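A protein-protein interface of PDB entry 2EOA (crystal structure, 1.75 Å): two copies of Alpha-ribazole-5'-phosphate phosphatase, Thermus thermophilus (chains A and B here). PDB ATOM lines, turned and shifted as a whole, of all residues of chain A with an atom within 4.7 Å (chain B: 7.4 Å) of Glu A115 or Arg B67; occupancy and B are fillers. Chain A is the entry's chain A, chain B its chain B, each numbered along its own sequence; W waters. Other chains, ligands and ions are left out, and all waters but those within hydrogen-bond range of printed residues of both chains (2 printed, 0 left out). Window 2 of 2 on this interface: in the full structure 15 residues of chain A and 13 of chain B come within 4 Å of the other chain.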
ATOM      1  N   SER A 111      -2.679 -13.966  20.120  1.00  0.00           N
ATOM      2  CA  SER A 111      -1.293 -14.119  20.564  1.00  0.00           C
ATOM      3  C   SER A 111      -1.240 -14.455  22.053  1.00  0.00           C
ATOM      4  O   SER A 111      -0.419 -15.267  22.488  1.00  0.00           O
ATOM      5  CB  SER A 111      -0.499 -12.831  20.304  1.00  0.00           C
ATOM      6  OG  SER A 111      -0.352 -12.583  18.917  1.00  0.00           O
ATOM      7  N   ALA A 112      -2.110 -13.820  22.836  1.00  0.00           N
ATOM      8  CA  ALA A 112      -2.148 -14.074  24.274  1.00  0.00           C
ATOM      9  C   ALA A 112      -2.662 -15.485  24.527  1.00  0.00           C
ATOM     10  O   ALA A 112      -2.171 -16.192  25.410  1.00  0.00           O
ATOM     11  CB  ALA A 112      -3.054 -13.060  24.967  1.00  0.00           C
ATOM     12  N   PHE A 113      -3.665 -15.871  23.744  1.00  0.00           N
ATOM     13  CA  PHE A 113      -4.288 -17.186  23.829  1.00  0.00           C
ATOM     14  C   PHE A 113      -3.251 -18.264  23.549  1.00  0.00           C
ATOM     15  O   PHE A 113      -3.098 -19.212  24.321  1.00  0.00           O
ATOM     16  CB  PHE A 113      -5.436 -17.264  22.808  1.00  0.00           C
ATOM     17  CG  PHE A 113      -6.063 -18.629  22.671  1.00  0.00           C
ATOM     18  CD1 PHE A 113      -6.659 -19.260  23.757  1.00  0.00           C
ATOM     19  CD2 PHE A 113      -6.091 -19.264  21.431  1.00  0.00           C
ATOM     20  CE1 PHE A 113      -7.282 -20.504  23.612  1.00  0.00           C
ATOM     21  CE2 PHE A 113      -6.707 -20.502  21.272  1.00  0.00           C
ATOM     22  CZ  PHE A 113      -7.305 -21.126  22.364  1.00  0.00           C
ATOM     23  N   GLN A 114      -2.534 -18.110  22.440  1.00  0.00           N
ATOM     24  CA  GLN A 114      -1.507 -19.079  22.064  1.00  0.00           C
ATOM     25  C   GLN A 114      -0.439 -19.193  23.149  1.00  0.00           C
ATOM     26  O   GLN A 114      -0.053 -20.295  23.540  1.00  0.00           O
ATOM     27  CB  GLN A 114      -0.865 -18.671  20.734  1.00  0.00           C
ATOM     28  CG  GLN A 114      -1.727 -18.988  19.513  1.00  0.00           C
ATOM     29  CD  GLN A 114      -1.236 -18.309  18.248  1.00  0.00           C
ATOM     30  OE1 GLN A 114      -1.426 -18.819  17.140  1.00  0.00           O
ATOM     31  NE2 GLN A 114      -0.613 -17.147  18.404  1.00  0.00           N
ATOM     32  N   GLU A 115       0.032 -18.053  23.645  1.00  0.00           N
ATOM     33  CA  GLU A 115       1.055 -18.065  24.683  1.00  0.00           C
ATOM     34  C   GLU A 115       0.573 -18.850  25.904  1.00  0.00           C
ATOM     35  O   GLU A 115       1.313 -19.659  26.462  1.00  0.00           O
ATOM     36  CB  GLU A 115       1.426 -16.629  25.079  1.00  0.00           C
ATOM     37  CG  GLU A 115       2.421 -16.539  26.227  1.00  0.00           C
ATOM     38  CD  GLU A 115       2.994 -15.141  26.398  1.00  0.00           C
ATOM     39  OE1 GLU A 115       2.236 -14.158  26.266  1.00  0.00           O
ATOM     40  OE2 GLU A 115       4.207 -15.027  26.674  1.00  0.00           O
ATOM     41  N   ARG A 116      -0.670 -18.609  26.305  1.00  0.00           N
ATOM     42  CA  ARG A 116      -1.279 -19.285  27.445  1.00  0.00           C
ATOM     43  C   ARG A 116      -1.332 -20.799  27.237  1.00  0.00           C
ATOM     44  O   ARG A 116      -0.902 -21.578  28.096  1.00  0.00           O
ATOM     45  CB  ARG A 116      -2.698 -18.736  27.664  1.00  0.00           C
ATOM     46  CG  ARG A 116      -3.603 -19.597  28.521  1.00  0.00           C
ATOM     47  CD  ARG A 116      -4.758 -18.781  29.099  1.00  0.00           C
ATOM     48  NE  ARG A 116      -5.819 -18.415  28.153  1.00  0.00           N
ATOM     49  CZ  ARG A 116      -6.721 -19.260  27.657  1.00  0.00           C
ATOM     50  NH1 ARG A 116      -6.697 -20.545  27.984  1.00  0.00           N
ATOM     51  NH2 ARG A 116      -7.708 -18.801  26.896  1.00  0.00           N
ATOM     52  N   VAL A 117      -1.863 -21.205  26.090  1.00  0.00           N
ATOM     53  CA  VAL A 117      -1.991 -22.616  25.760  1.00  0.00           C
ATOM     54  C   VAL A 117      -0.638 -23.307  25.655  1.00  0.00           C
ATOM     55  O   VAL A 117      -0.420 -24.357  26.260  1.00  0.00           O
ATOM     56  CB  VAL A 117      -2.756 -22.803  24.429  1.00  0.00           C
ATOM     57  CG1 VAL A 117      -2.708 -24.260  23.990  1.00  0.00           C
ATOM     58  CG2 VAL A 117      -4.203 -22.362  24.606  1.00  0.00           C
ATOM     59  N   PHE A 118       0.277 -22.718  24.899  1.00  0.00           N
ATOM     60  CA  PHE A 118       1.585 -23.342  24.726  1.00  0.00           C
ATOM     61  C   PHE A 118       2.420 -23.375  26.003  1.00  0.00           C
ATOM     62  O   PHE A 118       3.218 -24.293  26.199  1.00  0.00           O
ATOM     63  CB  PHE A 118       2.345 -22.659  23.590  1.00  0.00           C
ATOM     64  CG  PHE A 118       1.617 -22.707  22.273  1.00  0.00           C
ATOM     65  CD1 PHE A 118       0.842 -23.816  21.933  1.00  0.00           C
ATOM     66  CD2 PHE A 118       1.715 -21.659  21.367  1.00  0.00           C
ATOM     67  CE1 PHE A 118       0.171 -23.876  20.700  1.00  0.00           C
ATOM     68  CE2 PHE A 118       1.050 -21.710  20.134  1.00  0.00           C
ATOM     69  CZ  PHE A 118       0.278 -22.821  19.804  1.00  0.00           C
ATOM     70  N   ARG A 119       2.233 -22.387  26.874  1.00  0.00           N
ATOM     71  CA  ARG A 119       2.966 -22.358  28.136  1.00  0.00           C
ATOM     72  C   ARG A 119       2.456 -23.521  28.982  1.00  0.00           C
ATOM     73  O   ARG A 119       3.230 -24.206  29.655  1.00  0.00           O
ATOM     74  CB  ARG A 119       2.733 -21.034  28.873  1.00  0.00           C
ATOM     75  CG  ARG A 119       3.527 -20.910  30.166  1.00  0.00           C
ATOM     76  CD  ARG A 119       3.157 -19.642  30.920  1.00  0.00           C
ATOM     77  NE  ARG A 119       3.495 -18.433  30.173  1.00  0.00           N
ATOM     78  CZ  ARG A 119       4.734 -18.004  29.954  1.00  0.00           C
ATOM     79  NH1 ARG A 119       5.772 -18.685  30.427  1.00  0.00           N
ATOM     80  NH2 ARG A 119       4.937 -16.889  29.267  1.00  0.00           N
ATOM     81  N   PRO B  46       2.495 -19.873  14.200  1.00  0.00           N
ATOM     82  CA  PRO B  46       2.541 -18.632  14.981  1.00  0.00           C
ATOM     83  C   PRO B  46       3.722 -17.825  14.453  1.00  0.00           C
ATOM     84  O   PRO B  46       4.786 -18.391  14.179  1.00  0.00           O
ATOM     85  CB  PRO B  46       2.780 -19.132  16.402  1.00  0.00           C
ATOM     86  CG  PRO B  46       2.025 -20.416  16.424  1.00  0.00           C
ATOM     87  CD  PRO B  46       2.377 -21.046  15.086  1.00  0.00           C
ATOM     88  N   ALA B  47       3.549 -16.516  14.309  1.00  0.00           N
ATOM     89  CA  ALA B  47       4.618 -15.686  13.765  1.00  0.00           C
ATOM     90  C   ALA B  47       5.208 -14.696  14.751  1.00  0.00           C
ATOM     91  O   ALA B  47       4.509 -14.154  15.603  1.00  0.00           O
ATOM     92  CB  ALA B  47       4.114 -14.944  12.530  1.00  0.00           C
ATOM     93  N   PHE B  48       6.511 -14.477  14.614  1.00  0.00           N
ATOM     94  CA  PHE B  48       7.261 -13.542  15.445  1.00  0.00           C
ATOM     95  C   PHE B  48       8.114 -12.741  14.480  1.00  0.00           C
ATOM     96  O   PHE B  48       8.420 -13.201  13.383  1.00  0.00           O
ATOM     97  CB  PHE B  48       8.174 -14.293  16.413  1.00  0.00           C
ATOM     98  CG  PHE B  48       7.435 -15.096  17.437  1.00  0.00           C
ATOM     99  CD1 PHE B  48       7.046 -16.402  17.161  1.00  0.00           C
ATOM    100  CD2 PHE B  48       7.102 -14.541  18.666  1.00  0.00           C
ATOM    101  CE1 PHE B  48       6.331 -17.147  18.100  1.00  0.00           C
ATOM    102  CE2 PHE B  48       6.390 -15.278  19.611  1.00  0.00           C
ATOM    103  CZ  PHE B  48       6.003 -16.583  19.327  1.00  0.00           C
ATOM    104  N   SER B  49       8.512 -11.544  14.881  1.00  0.00           N
ATOM    105  CA  SER B  49       9.328 -10.740  13.994  1.00  0.00           C
ATOM    106  C   SER B  49      10.171  -9.730  14.738  1.00  0.00           C
ATOM    107  O   SER B  49       9.810  -9.273  15.823  1.00  0.00           O
ATOM    108  CB  SER B  49       8.435  -9.994  12.993  1.00  0.00           C
ATOM    109  OG  SER B  49       9.185  -9.078  12.207  1.00  0.00           O
ATOM    110  N   SER B  50      11.323  -9.424  14.154  1.00  0.00           N
ATOM    111  CA  SER B  50      12.195  -8.386  14.681  1.00  0.00           C
ATOM    112  C   SER B  50      11.283  -7.155  14.612  1.00  0.00           C
ATOM    113  O   SER B  50      10.399  -7.097  13.757  1.00  0.00           O
ATOM    114  CB  SER B  50      13.393  -8.216  13.740  1.00  0.00           C
ATOM    115  OG  SER B  50      13.960  -6.920  13.822  1.00  0.00           O
ATOM    116  N   ASP B  51      11.479  -6.180  15.495  1.00  0.00           N
ATOM    117  CA  ASP B  51      10.625  -4.994  15.474  1.00  0.00           C
ATOM    118  C   ASP B  51      11.050  -3.935  14.455  1.00  0.00           C
ATOM    119  O   ASP B  51      10.366  -2.924  14.285  1.00  0.00           O
ATOM    120  CB  ASP B  51      10.537  -4.378  16.875  1.00  0.00           C
ATOM    121  CG  ASP B  51      11.878  -3.923  17.399  1.00  0.00           C
ATOM    122  OD1 ASP B  51      12.866  -4.672  17.237  1.00  0.00           O
ATOM    123  OD2 ASP B  51      11.940  -2.817  17.985  1.00  0.00           O
ATOM    124  N   SER B  65       0.881 -11.609  10.886  1.00  0.00           N
ATOM    125  CA  SER B  65       0.649 -10.555  11.881  1.00  0.00           C
ATOM    126  C   SER B  65       1.485 -11.044  13.061  1.00  0.00           C
ATOM    127  O   SER B  65       0.978 -11.661  13.992  1.00  0.00           O
ATOM    128  CB  SER B  65      -0.831 -10.496  12.273  1.00  0.00           C
ATOM    129  OG  SER B  65      -1.645 -10.262  11.139  1.00  0.00           O
ATOM    130  N   PRO B  66       2.792 -10.763  13.033  1.00  0.00           N
ATOM    131  CA  PRO B  66       3.725 -11.191  14.075  1.00  0.00           C
ATOM    132  C   PRO B  66       3.774 -10.483  15.414  1.00  0.00           C
ATOM    133  O   PRO B  66       3.456  -9.299  15.523  1.00  0.00           O
ATOM    134  CB  PRO B  66       5.068 -11.093  13.366  1.00  0.00           C
ATOM    135  CG  PRO B  66       4.897  -9.806  12.600  1.00  0.00           C
ATOM    136  CD  PRO B  66       3.481  -9.944  12.017  1.00  0.00           C
ATOM    137  N   ARG B  67       4.187 -11.238  16.429  1.00  0.00           N
ATOM    138  CA  ARG B  67       4.400 -10.700  17.766  1.00  0.00           C
ATOM    139  C   ARG B  67       5.813 -10.143  17.605  1.00  0.00           C
ATOM    140  O   ARG B  67       6.702 -10.833  17.098  1.00  0.00           O
ATOM    141  CB  ARG B  67       4.370 -11.821  18.809  1.00  0.00           C
ATOM    142  CG  ARG B  67       2.983 -12.400  19.027  1.00  0.00           C
ATOM    143  CD  ARG B  67       3.016 -13.717  19.806  1.00  0.00           C
ATOM    144  NE  ARG B  67       3.634 -13.584  21.121  1.00  0.00           N
ATOM    145  CZ  ARG B  67       3.748 -14.581  21.993  1.00  0.00           C
ATOM    146  NH1 ARG B  67       3.282 -15.787  21.693  1.00  0.00           N
ATOM    147  NH2 ARG B  67       4.332 -14.375  23.166  1.00  0.00           N
ATOM    148  N   LEU B  68       6.015  -8.892  18.010  1.00  0.00           N
ATOM    149  CA  LEU B  68       7.306  -8.237  17.856  1.00  0.00           C
ATOM    150  C   LEU B  68       8.265  -8.433  19.020  1.00  0.00           C
ATOM    151  O   LEU B  68       7.903  -8.243  20.180  1.00  0.00           O
ATOM    152  CB  LEU B  68       7.092  -6.738  17.604  1.00  0.00           C
ATOM    153  CG  LEU B  68       6.154  -6.363  16.449  1.00  0.00           C
ATOM    154  CD1 LEU B  68       6.106  -4.846  16.300  1.00  0.00           C
ATOM    155  CD2 LEU B  68       6.631  -7.005  15.156  1.00  0.00           C
ATOM    156  N   TYR B  69       9.500  -8.801  18.690  1.00  0.00           N
ATOM    157  CA  TYR B  69      10.548  -9.034  19.680  1.00  0.00           C
ATOM    158  C   TYR B  69      11.872  -8.438  19.236  1.00  0.00           C
ATOM    159  O   TYR B  69      12.423  -8.827  18.205  1.00  0.00           O
ATOM    160  CB  TYR B  69      10.740 -10.536  19.904  1.00  0.00           C
ATOM    161  CG  TYR B  69       9.715 -11.152  20.817  1.00  0.00           C
ATOM    162  CD1 TYR B  69       8.433 -11.455  20.355  1.00  0.00           C
ATOM    163  CD2 TYR B  69      10.017 -11.415  22.156  1.00  0.00           C
ATOM    164  CE1 TYR B  69       7.479 -12.001  21.202  1.00  0.00           C
ATOM    165  CE2 TYR B  69       9.067 -11.965  23.010  1.00  0.00           C
ATOM    166  CZ  TYR B  69       7.802 -12.252  22.528  1.00  0.00           C
ATOM    167  OH  TYR B  69       6.858 -12.784  23.376  1.00  0.00           O
ATOM    168  N   PRO B  70      12.404  -7.481  20.007  1.00  0.00           N
ATOM    169  CA  PRO B  70      13.683  -6.874  19.631  1.00  0.00           C
ATOM    170  C   PRO B  70      14.813  -7.901  19.654  1.00  0.00           C
ATOM    171  O   PRO B  70      15.855  -7.701  19.036  1.00  0.00           O
ATOM    172  CB  PRO B  70      13.865  -5.780  20.683  1.00  0.00           C
ATOM    173  CG  PRO B  70      12.456  -5.378  20.985  1.00  0.00           C
ATOM    174  CD  PRO B  70      11.760  -6.720  21.093  1.00  0.00           C
ATOM    175  N   LEU B  72      15.016 -10.454  18.133  1.00  0.00           N
ATOM    176  CA  LEU B  72      15.200 -10.967  16.776  1.00  0.00           C
ATOM    177  C   LEU B  72      15.907  -9.988  15.845  1.00  0.00           C
ATOM    178  O   LEU B  72      16.047 -10.249  14.653  1.00  0.00           O
ATOM    179  CB  LEU B  72      13.850 -11.365  16.169  1.00  0.00           C
ATOM    180  CG  LEU B  72      13.279 -12.712  16.628  1.00  0.00           C
ATOM    181  CD1 LEU B  72      11.876 -12.890  16.052  1.00  0.00           C
ATOM    182  CD2 LEU B  72      14.208 -13.841  16.170  1.00  0.00           C
ATOM    183  N   PHE B 120      16.139 -16.171  23.059  1.00  0.00           N
ATOM    184  CA  PHE B 120      14.826 -16.060  22.445  1.00  0.00           C
ATOM    185  C   PHE B 120      14.388 -17.416  21.899  1.00  0.00           C
ATOM    186  O   PHE B 120      13.272 -17.865  22.155  1.00  0.00           O
ATOM    187  CB  PHE B 120      14.840 -15.059  21.290  1.00  0.00           C
ATOM    188  CG  PHE B 120      13.540 -14.998  20.541  1.00  0.00           C
ATOM    189  CD1 PHE B 120      12.445 -14.320  21.070  1.00  0.00           C
ATOM    190  CD2 PHE B 120      13.389 -15.669  19.330  1.00  0.00           C
ATOM    191  CE1 PHE B 120      11.217 -14.311  20.404  1.00  0.00           C
ATOM    192  CE2 PHE B 120      12.165 -15.668  18.656  1.00  0.00           C
ATOM    193  CZ  PHE B 120      11.077 -14.986  19.196  1.00  0.00           C
ATOM    194  N   LEU B 124      11.020 -20.222  22.928  1.00  0.00           N
ATOM    195  CA  LEU B 124       9.865 -20.580  22.106  1.00  0.00           C
ATOM    196  C   LEU B 124       9.191 -21.850  22.636  1.00  0.00           C
ATOM    197  O   LEU B 124       9.864 -22.796  23.041  1.00  0.00           O
ATOM    198  CB  LEU B 124      10.299 -20.759  20.647  1.00  0.00           C
ATOM    199  CG  LEU B 124      10.716 -19.458  19.948  1.00  0.00           C
ATOM    200  CD1 LEU B 124      11.350 -19.758  18.589  1.00  0.00           C
ATOM    201  CD2 LEU B 124       9.492 -18.558  19.775  1.00  0.00           C
ATOM    202  N   LYS B 125       7.861 -21.865  22.621  1.00  0.00           N
ATOM    203  CA  LYS B 125       7.099 -22.993  23.143  1.00  0.00           C
ATOM    204  C   LYS B 125       6.279 -23.754  22.107  1.00  0.00           C
ATOM    205  O   LYS B 125       5.505 -24.642  22.456  1.00  0.00           O
ATOM    206  CB  LYS B 125       6.180 -22.501  24.263  1.00  0.00           C
ATOM    207  CG  LYS B 125       6.938 -21.820  25.391  1.00  0.00           C
ATOM    208  CD  LYS B 125       6.012 -21.197  26.416  1.00  0.00           C
ATOM    209  CE  LYS B 125       6.820 -20.560  27.538  1.00  0.00           C
ATOM    210  NZ  LYS B 125       7.795 -19.562  27.006  1.00  0.00           N
ATOM    211  N   VAL B 129       7.178 -19.128  12.724  1.00  0.00           N
ATOM    212  CA  VAL B 129       7.822 -18.521  11.567  1.00  0.00           C
ATOM    213  C   VAL B 129       8.453 -17.273  12.173  1.00  0.00           C
ATOM    214  O   VAL B 129       7.770 -16.493  12.848  1.00  0.00           O
ATOM    215  CB  VAL B 129       6.809 -18.120  10.473  1.00  0.00           C
ATOM    216  CG1 VAL B 129       7.524 -17.339   9.366  1.00  0.00           C
ATOM    217  CG2 VAL B 129       6.158 -19.376   9.881  1.00  0.00           C
ATOM    218  N   PHE B 131      10.455 -13.810  11.400  1.00  0.00           N
ATOM    219  CA  PHE B 131      10.894 -12.819  10.425  1.00  0.00           C
ATOM    220  C   PHE B 131      12.053 -12.086  11.062  1.00  0.00           C
ATOM    221  O   PHE B 131      11.886 -11.352  12.036  1.00  0.00           O
ATOM    222  CB  PHE B 131       9.737 -11.885  10.080  1.00  0.00           C
ATOM    223  CG  PHE B 131       8.698 -12.545   9.240  1.00  0.00           C
ATOM    224  CD1 PHE B 131       8.867 -12.650   7.863  1.00  0.00           C
ATOM    225  CD2 PHE B 131       7.599 -13.163   9.828  1.00  0.00           C
ATOM    226  CE1 PHE B 131       7.963 -13.365   7.087  1.00  0.00           C
ATOM    227  CE2 PHE B 131       6.688 -13.880   9.059  1.00  0.00           C
ATOM    228  CZ  PHE B 131       6.871 -13.984   7.687  1.00  0.00           C
HETATM  229  O   HOH W   1       1.878 -16.663  19.342  1.00  0.00           O
HETATM  230  O   HOH W   2       4.818 -25.924  24.629  1.00  0.00           O
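The guanidinium group (NH2) of Arg B67 is in salt-bridge range of the side-chain carboxylate (OE2) of Glu A115, 3.6 Å away.
The side-chain carboxylate (OE2) of Glu A115 lies within salt-bridge range of the guanidinium group (NH2) of Arg A119 (3.3 Å). The backbone NH (N) of Val B129 is in hydrogen-bond range of the backbone carbonyl oxygen (O) of Pro B46 (2.9 Å). The backbone carbonyl oxygen (O) of Ala B47 is in hydrogen-bond range of the backbone NH (N) of Arg B67 (3.0 Å). N of Ser B49 lies within hydrogen-bond range of O of Arg B67. The guanidinium group (NH2) of Arg B67 lies within hydrogen-bond range of the side-chain hydroxyl (OH) of Tyr B69, 3.0 Å away.
Ser A111 touches Arg B67 (OG to CG, 3.3 Å). Pro B46 touches Gln A114. CB of Lys B125 touches CB of Phe A118, at 3.9 Å. NH1 of Arg A119 touches CE of Lys B125, 3.6 Å away.
Glu A115 touches one residue of chain B. Arg B67 touches two residues of chain A. Of the printed residues of chain B, Phe A118 touches Lys B125. Of the printed residues of chain B, Ser A111 touches Arg B67. Of the printed residues of chain A, Lys B125 touches Phe A118 (3.9 Å) and Arg A119 (3.6 Å). Of the printed residues of chain B, Arg A119 touches Lys B125 (3.6 Å). Printed residues of chain A within 4 Å of Pro B46: Gln A114. Ser B49 touches none of the printed residues of chain A. Val B129 touches none of the printed residues of chain A. The nearest residue of chain B that does not touch Glu A115 is Tyr B69 (4.8 Å). The nearest printed residue of chain A that does not touch Arg B67 is Gln A114 (5.1 Å). The nearest printed residue of chain A that does not touch Lys B125 is Glu A115 (4.9 Å).
Of the 18 printed residues of chain B, 3 touch a printed residue of chain A. Printed residues of chain B that touch a printed residue of chain A: Pro B46, Arg B67 and Lys B125. Hydrophobic or aromatic side chains of chain B that line the printed part of chain A: Pro B46. Hydrophobic or aromatic side chains of chain A within 4 Å of the printed part of chain B: Phe A118. Among the printed residues, 5 pairs touch across the chains. Among the printed residues, Asp or Glu carboxylates within 4 Å of a Lys or Arg side-chain nitrogen of the other chain: Glu A115 with Arg B67 (3.6 Å).
No position is printed for both chains.
Water W2 bridges the backbone carbonyl oxygen (O) of Lys B125 (2.6 Å) and the backbone carbonyl oxygen (O) of Phe A118 (2.8 Å). Water W1 lies within hydrogen-bond range of the side-chain amide nitrogen (NE2) of Gln A114 (2.7 Å) and the guanidinium group (NH1) of Arg B67 (2.9 Å).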
